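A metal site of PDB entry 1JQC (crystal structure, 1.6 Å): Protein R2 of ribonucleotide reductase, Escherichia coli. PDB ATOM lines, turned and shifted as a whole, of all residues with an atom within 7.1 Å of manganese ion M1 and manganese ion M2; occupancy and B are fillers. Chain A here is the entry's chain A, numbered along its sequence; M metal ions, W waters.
The side-chain hydroxyl of Ser 114 sits at hydrogen-bond distance from a ring nitrogen (NE2) of His 241.
OG of Ser 114 lies within hydrogen-bond range of O of Trp 111, at 2.7 Å.
The side-chain hydroxyl (OG) of Ser 119 lies within hydrogen-bond range of the backbone carbonyl oxygen (O) of Glu 115 (3.4 Å).
NE2 of His 118 lies within hydrogen-bond range of OD2 of Asp 237 (2.7 Å).
NE1 of Trp 111 sits close to OE2 of Glu 204, 2.9 Å away.
The side-chain hydroxyl (OH) of Tyr 122 is in hydrogen-bond range of the side-chain carboxylate (OD2) of Asp 84 (2.5 Å).
The side-chain hydroxyl of Ser 119 lies within hydrogen-bond range of the backbone carbonyl oxygen of Asp 84, 3.5 Å away.
A ring nitrogen (NE2) of His 241 lies close to the backbone carbonyl oxygen (O) of Asp 237, 3.5 Å away.
Four residues have an atom within 4 Å of manganese ion M1: Asp 84, Glu 115, His 118 and Glu 238.
The nearest printed residue that does not touch manganese ion M1 is Phe 208 (4.1 Å).
Residues that only touch manganese ion M2: Trp 111.
Manganese ion M1 is bound by OD1 of Asp 84, OE1 of Glu 115, ND1 of His 118, water W1 and OE2 of Glu 238.
Manganese ion M1 has five donor atoms within binding distance.
Manganese ion M2 is bound by OE1 of Glu 238 (1.9 Å), OE2 of Glu 204 (2.1 Å), OE2 of Glu 115 (2.1 Å), OE2 of Glu 238 (2.2 Å), ND1 of His 241 (2.3 Å) and water W2 (2.3 Å).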
ATOM      1  N   GLN A  80     -27.717  11.708  14.697  1.00  0.00           N
ATOM      2  CA  GLN A  80     -26.977  12.971  14.598  1.00  0.00           C
ATOM      3  C   GLN A  80     -27.949  14.143  14.711  1.00  0.00           C
ATOM      4  O   GLN A  80     -27.679  15.140  15.425  1.00  0.00           O
ATOM      5  CB  GLN A  80     -26.221  13.037  13.247  1.00  0.00           C
ATOM      6  CG  GLN A  80     -25.123  11.928  13.205  1.00  0.00           C
ATOM      7  CD  GLN A  80     -24.432  11.777  11.856  1.00  0.00           C
ATOM      8  OE1 GLN A  80     -25.039  11.964  10.798  1.00  0.00           O
ATOM      9  NE2 GLN A  80     -23.145  11.421  11.906  1.00  0.00           N
ATOM     10  N   LEU A  83     -29.081  14.574  18.380  1.00  0.00           N
ATOM     11  CA  LEU A  83     -28.048  15.185  19.214  1.00  0.00           C
ATOM     12  C   LEU A  83     -27.851  16.683  18.947  1.00  0.00           C
ATOM     13  O   LEU A  83     -27.753  17.492  19.910  1.00  0.00           O
ATOM     14  CB  LEU A  83     -26.720  14.432  19.029  1.00  0.00           C
ATOM     15  CG  LEU A  83     -26.716  13.026  19.665  1.00  0.00           C
ATOM     16  CD1 LEU A  83     -25.304  12.512  19.548  1.00  0.00           C
ATOM     17  CD2 LEU A  83     -27.098  13.024  21.124  1.00  0.00           C
ATOM     18  N   ASP A  84     -27.856  17.094  17.674  1.00  0.00           N
ATOM     19  CA  ASP A  84     -27.631  18.499  17.354  1.00  0.00           C
ATOM     20  C   ASP A  84     -28.876  19.331  17.652  1.00  0.00           C
ATOM     21  O   ASP A  84     -28.752  20.530  17.895  1.00  0.00           O
ATOM     22  CB  ASP A  84     -27.165  18.725  15.900  1.00  0.00           C
ATOM     23  CG  ASP A  84     -25.644  18.541  15.731  1.00  0.00           C
ATOM     24  OD1 ASP A  84     -24.882  19.260  16.377  1.00  0.00           O
ATOM     25  OD2 ASP A  84     -25.181  17.671  14.942  1.00  0.00           O
ATOM     26  N   GLN A  87     -28.239  19.946  21.189  1.00  0.00           N
ATOM     27  CA  GLN A  87     -27.078  20.809  21.392  1.00  0.00           C
ATOM     28  C   GLN A  87     -27.244  22.226  20.857  1.00  0.00           C
ATOM     29  O   GLN A  87     -26.497  23.111  21.295  1.00  0.00           O
ATOM     30  CB  GLN A  87     -25.821  20.171  20.773  1.00  0.00           C
ATOM     31  CG  GLN A  87     -25.394  18.931  21.571  1.00  0.00           C
ATOM     32  CD  GLN A  87     -24.961  19.335  22.986  1.00  0.00           C
ATOM     33  OE1 GLN A  87     -23.813  19.742  23.196  1.00  0.00           O
ATOM     34  NE2 GLN A  87     -25.858  19.239  23.893  1.00  0.00           N
ATOM     35  N   GLY A  88     -28.193  22.456  19.960  1.00  0.00           N
ATOM     36  CA  GLY A  88     -28.389  23.840  19.501  1.00  0.00           C
ATOM     37  C   GLY A  88     -29.004  24.706  20.596  1.00  0.00           C
ATOM     38  O   GLY A  88     -28.583  25.845  20.830  1.00  0.00           O
ATOM     39  N   TRP A 111     -20.746  28.333  20.185  1.00  0.00           N
ATOM     40  CA  TRP A 111     -20.812  26.897  20.113  1.00  0.00           C
ATOM     41  C   TRP A 111     -22.275  26.473  19.817  1.00  0.00           C
ATOM     42  O   TRP A 111     -22.519  25.712  18.875  1.00  0.00           O
ATOM     43  CB  TRP A 111     -20.356  26.381  21.493  1.00  0.00           C
ATOM     44  CG  TRP A 111     -20.630  24.933  21.852  1.00  0.00           C
ATOM     45  CD1 TRP A 111     -20.915  23.877  21.028  1.00  0.00           C
ATOM     46  CD2 TRP A 111     -20.575  24.414  23.180  1.00  0.00           C
ATOM     47  NE1 TRP A 111     -21.031  22.718  21.799  1.00  0.00           N
ATOM     48  CE2 TRP A 111     -20.830  23.046  23.123  1.00  0.00           C
ATOM     49  CE3 TRP A 111     -20.344  25.012  24.439  1.00  0.00           C
ATOM     50  CZ2 TRP A 111     -20.849  22.240  24.288  1.00  0.00           C
ATOM     51  CZ3 TRP A 111     -20.378  24.238  25.582  1.00  0.00           C
ATOM     52  CH2 TRP A 111     -20.629  22.860  25.499  1.00  0.00           C
ATOM     53  N   SER A 114     -23.254  27.210  16.298  1.00  0.00           N
ATOM     54  CA  SER A 114     -22.620  26.306  15.342  1.00  0.00           C
ATOM     55  C   SER A 114     -23.401  24.982  15.267  1.00  0.00           C
ATOM     56  O   SER A 114     -23.476  24.371  14.203  1.00  0.00           O
ATOM     57  CB  SER A 114     -21.118  26.111  15.676  1.00  0.00           C
ATOM     58  OG  SER A 114     -20.954  25.194  16.726  1.00  0.00           O
ATOM     59  N   GLU A 115     -24.063  24.570  16.365  1.00  0.00           N
ATOM     60  CA  GLU A 115     -24.845  23.347  16.344  1.00  0.00           C
ATOM     61  C   GLU A 115     -26.132  23.541  15.494  1.00  0.00           C
ATOM     62  O   GLU A 115     -26.614  22.580  14.865  1.00  0.00           O
ATOM     63  CB  GLU A 115     -25.241  22.951  17.772  1.00  0.00           C
ATOM     64  CG  GLU A 115     -24.088  22.789  18.788  1.00  0.00           C
ATOM     65  CD  GLU A 115     -23.174  21.635  18.538  1.00  0.00           C
ATOM     66  OE1 GLU A 115     -23.043  21.253  17.359  1.00  0.00           O
ATOM     67  OE2 GLU A 115     -22.568  21.154  19.477  1.00  0.00           O
ATOM     68  N   THR A 116     -26.704  24.753  15.477  1.00  0.00           N
ATOM     69  CA  THR A 116     -27.889  25.000  14.637  1.00  0.00           C
ATOM     70  C   THR A 116     -27.489  24.885  13.179  1.00  0.00           C
ATOM     71  O   THR A 116     -28.316  24.506  12.373  1.00  0.00           O
ATOM     72  CB  THR A 116     -28.582  26.390  14.887  1.00  0.00           C
ATOM     73  OG1 THR A 116     -27.740  27.451  14.420  1.00  0.00           O
ATOM     74  CG2 THR A 116     -28.867  26.555  16.420  1.00  0.00           C
ATOM     75  N   HIS A 118     -25.265  22.769  12.163  1.00  0.00           N
ATOM     76  CA  HIS A 118     -25.234  21.298  11.944  1.00  0.00           C
ATOM     77  C   HIS A 118     -26.674  20.810  11.697  1.00  0.00           C
ATOM     78  O   HIS A 118     -26.936  20.010  10.751  1.00  0.00           O
ATOM     79  CB  HIS A 118     -24.612  20.581  13.163  1.00  0.00           C
ATOM     80  CG  HIS A 118     -23.208  20.985  13.420  1.00  0.00           C
ATOM     81  ND1 HIS A 118     -22.496  20.547  14.504  1.00  0.00           N
ATOM     82  CD2 HIS A 118     -22.383  21.778  12.716  1.00  0.00           C
ATOM     83  CE1 HIS A 118     -21.282  21.053  14.451  1.00  0.00           C
ATOM     84  NE2 HIS A 118     -21.193  21.804  13.379  1.00  0.00           N
ATOM     85  N   SER A 119     -27.643  21.254  12.500  1.00  0.00           N
ATOM     86  CA  SER A 119     -29.016  20.817  12.252  1.00  0.00           C
ATOM     87  C   SER A 119     -29.500  21.201  10.864  1.00  0.00           C
ATOM     88  O   SER A 119     -30.204  20.429  10.215  1.00  0.00           O
ATOM     89  CB  SER A 119     -29.966  21.444  13.301  1.00  0.00           C
ATOM     90  OG  SER A 119     -29.615  20.980  14.577  1.00  0.00           O
ATOM     91  N   TYR A 122     -28.362  18.779   8.300  1.00  0.00           N
ATOM     92  CA  TYR A 122     -29.114  17.512   8.208  1.00  0.00           C
ATOM     93  C   TYR A 122     -30.404  17.708   7.418  1.00  0.00           C
ATOM     94  O   TYR A 122     -30.822  16.795   6.704  1.00  0.00           O
ATOM     95  CB  TYR A 122     -29.445  16.946   9.588  1.00  0.00           C
ATOM     96  CG  TYR A 122     -28.220  16.786  10.454  1.00  0.00           C
ATOM     97  CD1 TYR A 122     -27.045  16.213   9.936  1.00  0.00           C
ATOM     98  CD2 TYR A 122     -28.234  17.197  11.792  1.00  0.00           C
ATOM     99  CE1 TYR A 122     -25.907  16.056  10.757  1.00  0.00           C
ATOM    100  CE2 TYR A 122     -27.138  17.033  12.595  1.00  0.00           C
ATOM    101  CZ  TYR A 122     -25.976  16.479  12.105  1.00  0.00           C
ATOM    102  OH  TYR A 122     -24.864  16.284  12.930  1.00  0.00           O
ATOM    103  N   VAL A 200     -21.771  16.369  28.696  1.00  0.00           N
ATOM    104  CA  VAL A 200     -21.628  17.023  27.379  1.00  0.00           C
ATOM    105  C   VAL A 200     -20.298  16.627  26.734  1.00  0.00           C
ATOM    106  O   VAL A 200     -20.221  16.367  25.509  1.00  0.00           O
ATOM    107  CB  VAL A 200     -21.699  18.543  27.527  1.00  0.00           C
ATOM    108  CG1 VAL A 200     -21.514  19.234  26.164  1.00  0.00           C
ATOM    109  CG2 VAL A 200     -23.058  18.921  28.091  1.00  0.00           C
ATOM    110  N   LEU A 203     -20.818  13.360  25.249  1.00  0.00           N
ATOM    111  CA  LEU A 203     -21.650  13.475  24.107  1.00  0.00           C
ATOM    112  C   LEU A 203     -20.828  13.939  22.900  1.00  0.00           C
ATOM    113  O   LEU A 203     -20.889  13.328  21.853  1.00  0.00           O
ATOM    114  CB  LEU A 203     -22.767  14.506  24.403  1.00  0.00           C
ATOM    115  CG  LEU A 203     -23.874  14.696  23.345  1.00  0.00           C
ATOM    116  CD1 LEU A 203     -24.994  15.516  24.024  1.00  0.00           C
ATOM    117  CD2 LEU A 203     -23.409  15.500  22.081  1.00  0.00           C
ATOM    118  N   GLU A 204     -20.040  14.987  23.055  1.00  0.00           N
ATOM    119  CA  GLU A 204     -19.400  15.423  21.816  1.00  0.00           C
ATOM    120  C   GLU A 204     -18.157  14.631  21.480  1.00  0.00           C
ATOM    121  O   GLU A 204     -17.831  14.445  20.303  1.00  0.00           O
ATOM    122  CB  GLU A 204     -19.127  16.907  21.900  1.00  0.00           C
ATOM    123  CG  GLU A 204     -20.441  17.687  21.925  1.00  0.00           C
ATOM    124  CD  GLU A 204     -20.219  19.146  21.981  1.00  0.00           C
ATOM    125  OE1 GLU A 204     -19.402  19.562  22.801  1.00  0.00           O
ATOM    126  OE2 GLU A 204     -20.899  19.863  21.233  1.00  0.00           O
ATOM    127  N   PHE A 208     -20.758  11.490  19.265  1.00  0.00           N
ATOM    128  CA  PHE A 208     -20.702  12.012  17.899  1.00  0.00           C
ATOM    129  C   PHE A 208     -19.627  11.325  17.058  1.00  0.00           C
ATOM    130  O   PHE A 208     -19.839  11.098  15.854  1.00  0.00           O
ATOM    131  CB  PHE A 208     -20.498  13.520  17.896  1.00  0.00           C
ATOM    132  CG  PHE A 208     -21.724  14.268  17.489  1.00  0.00           C
ATOM    133  CD1 PHE A 208     -22.310  13.988  16.256  1.00  0.00           C
ATOM    134  CD2 PHE A 208     -22.361  15.144  18.349  1.00  0.00           C
ATOM    135  CE1 PHE A 208     -23.528  14.570  15.874  1.00  0.00           C
ATOM    136  CE2 PHE A 208     -23.582  15.736  17.992  1.00  0.00           C
ATOM    137  CZ  PHE A 208     -24.164  15.442  16.751  1.00  0.00           C
ATOM    138  N   PHE A 212     -19.699   9.492  13.417  1.00  0.00           N
ATOM    139  CA  PHE A 212     -18.854   9.939  12.288  1.00  0.00           C
ATOM    140  C   PHE A 212     -18.306   8.699  11.573  1.00  0.00           C
ATOM    141  O   PHE A 212     -18.258   8.628  10.312  1.00  0.00           O
ATOM    142  CB  PHE A 212     -17.690  10.822  12.782  1.00  0.00           C
ATOM    143  CG  PHE A 212     -18.114  12.142  13.371  1.00  0.00           C
ATOM    144  CD1 PHE A 212     -19.332  12.716  13.022  1.00  0.00           C
ATOM    145  CD2 PHE A 212     -17.290  12.805  14.276  1.00  0.00           C
ATOM    146  CE1 PHE A 212     -19.717  13.957  13.555  1.00  0.00           C
ATOM    147  CE2 PHE A 212     -17.700  14.083  14.807  1.00  0.00           C
ATOM    148  CZ  PHE A 212     -18.896  14.611  14.440  1.00  0.00           C
ATOM    149  N   ILE A 234     -18.640  19.184  10.002  1.00  0.00           N
ATOM    150  CA  ILE A 234     -19.212  19.034  11.382  1.00  0.00           C
ATOM    151  C   ILE A 234     -18.168  18.505  12.358  1.00  0.00           C
ATOM    152  O   ILE A 234     -18.039  19.008  13.531  1.00  0.00           O
ATOM    153  CB  ILE A 234     -20.443  18.106  11.337  1.00  0.00           C
ATOM    154  CG1 ILE A 234     -21.580  18.824  10.611  1.00  0.00           C
ATOM    155  CG2 ILE A 234     -20.903  17.669  12.816  1.00  0.00           C
ATOM    156  CD1 ILE A 234     -22.830  17.949  10.491  1.00  0.00           C
ATOM    157  N   ASP A 237     -15.859  21.084  13.604  1.00  0.00           N
ATOM    158  CA  ASP A 237     -16.483  21.910  14.659  1.00  0.00           C
ATOM    159  C   ASP A 237     -16.521  21.148  15.971  1.00  0.00           C
ATOM    160  O   ASP A 237     -16.224  21.703  17.028  1.00  0.00           O
ATOM    161  CB  ASP A 237     -17.934  22.299  14.306  1.00  0.00           C
ATOM    162  CG  ASP A 237     -18.033  23.240  13.112  1.00  0.00           C
ATOM    163  OD1 ASP A 237     -17.069  23.991  12.840  1.00  0.00           O
ATOM    164  OD2 ASP A 237     -19.121  23.260  12.523  1.00  0.00           O
ATOM    165  N   GLU A 238     -16.911  19.868  15.916  1.00  0.00           N
ATOM    166  CA  GLU A 238     -17.005  19.108  17.159  1.00  0.00           C
ATOM    167  C   GLU A 238     -15.675  19.015  17.879  1.00  0.00           C
ATOM    168  O   GLU A 238     -15.632  18.978  19.117  1.00  0.00           O
ATOM    169  CB  GLU A 238     -17.567  17.688  16.901  1.00  0.00           C
ATOM    170  CG  GLU A 238     -19.102  17.718  16.539  1.00  0.00           C
ATOM    171  CD  GLU A 238     -19.907  18.628  17.506  1.00  0.00           C
ATOM    172  OE1 GLU A 238     -19.599  18.563  18.726  1.00  0.00           O
ATOM    173  OE2 GLU A 238     -20.830  19.377  17.045  1.00  0.00           O
ATOM    174  N   ALA A 239     -14.555  18.973  17.117  1.00  0.00           N
ATOM    175  CA  ALA A 239     -13.229  18.910  17.749  1.00  0.00           C
ATOM    176  C   ALA A 239     -13.047  20.174  18.602  1.00  0.00           C
ATOM    177  O   ALA A 239     -12.481  20.124  19.695  1.00  0.00           O
ATOM    178  CB  ALA A 239     -12.135  18.803  16.657  1.00  0.00           C
ATOM    179  N   HIS A 241     -15.534  21.912  19.947  1.00  0.00           N
ATOM    180  CA  HIS A 241     -16.494  21.829  21.061  1.00  0.00           C
ATOM    181  C   HIS A 241     -15.948  20.953  22.183  1.00  0.00           C
ATOM    182  O   HIS A 241     -16.025  21.301  23.353  1.00  0.00           O
ATOM    183  CB  HIS A 241     -17.849  21.287  20.573  1.00  0.00           C
ATOM    184  CG  HIS A 241     -18.454  22.104  19.479  1.00  0.00           C
ATOM    185  ND1 HIS A 241     -19.575  21.684  18.759  1.00  0.00           N
ATOM    186  CD2 HIS A 241     -18.092  23.288  18.964  1.00  0.00           C
ATOM    187  CE1 HIS A 241     -19.869  22.620  17.866  1.00  0.00           C
ATOM    188  NE2 HIS A 241     -18.990  23.590  17.964  1.00  0.00           N
ATOM    189  N   LEU A 242     -15.413  19.802  21.829  1.00  0.00           N
ATOM    190  CA  LEU A 242     -14.891  18.944  22.903  1.00  0.00           C
ATOM    191  C   LEU A 242     -13.606  19.559  23.506  1.00  0.00           C
ATOM    192  O   LEU A 242     -13.290  19.363  24.700  1.00  0.00           O
ATOM    193  CB  LEU A 242     -14.690  17.524  22.348  1.00  0.00           C
ATOM    194  CG  LEU A 242     -13.567  17.346  21.363  1.00  0.00           C
ATOM    195  CD1 LEU A 242     -12.307  16.994  22.146  1.00  0.00           C
ATOM    196  CD2 LEU A 242     -13.900  16.195  20.393  1.00  0.00           C
HETATM  197 MN    MN M   1     -22.926  19.446  16.348  1.00  0.00          MN
HETATM  198 MN    MN M   2     -20.939  19.895  19.166  1.00  0.00          MN
HETATM  199  O   HOH W   1     -22.379  17.453  15.585  1.00  0.00           O
HETATM  200  O   HOH W   2     -22.588  18.285  19.106  1.00  0.00           O
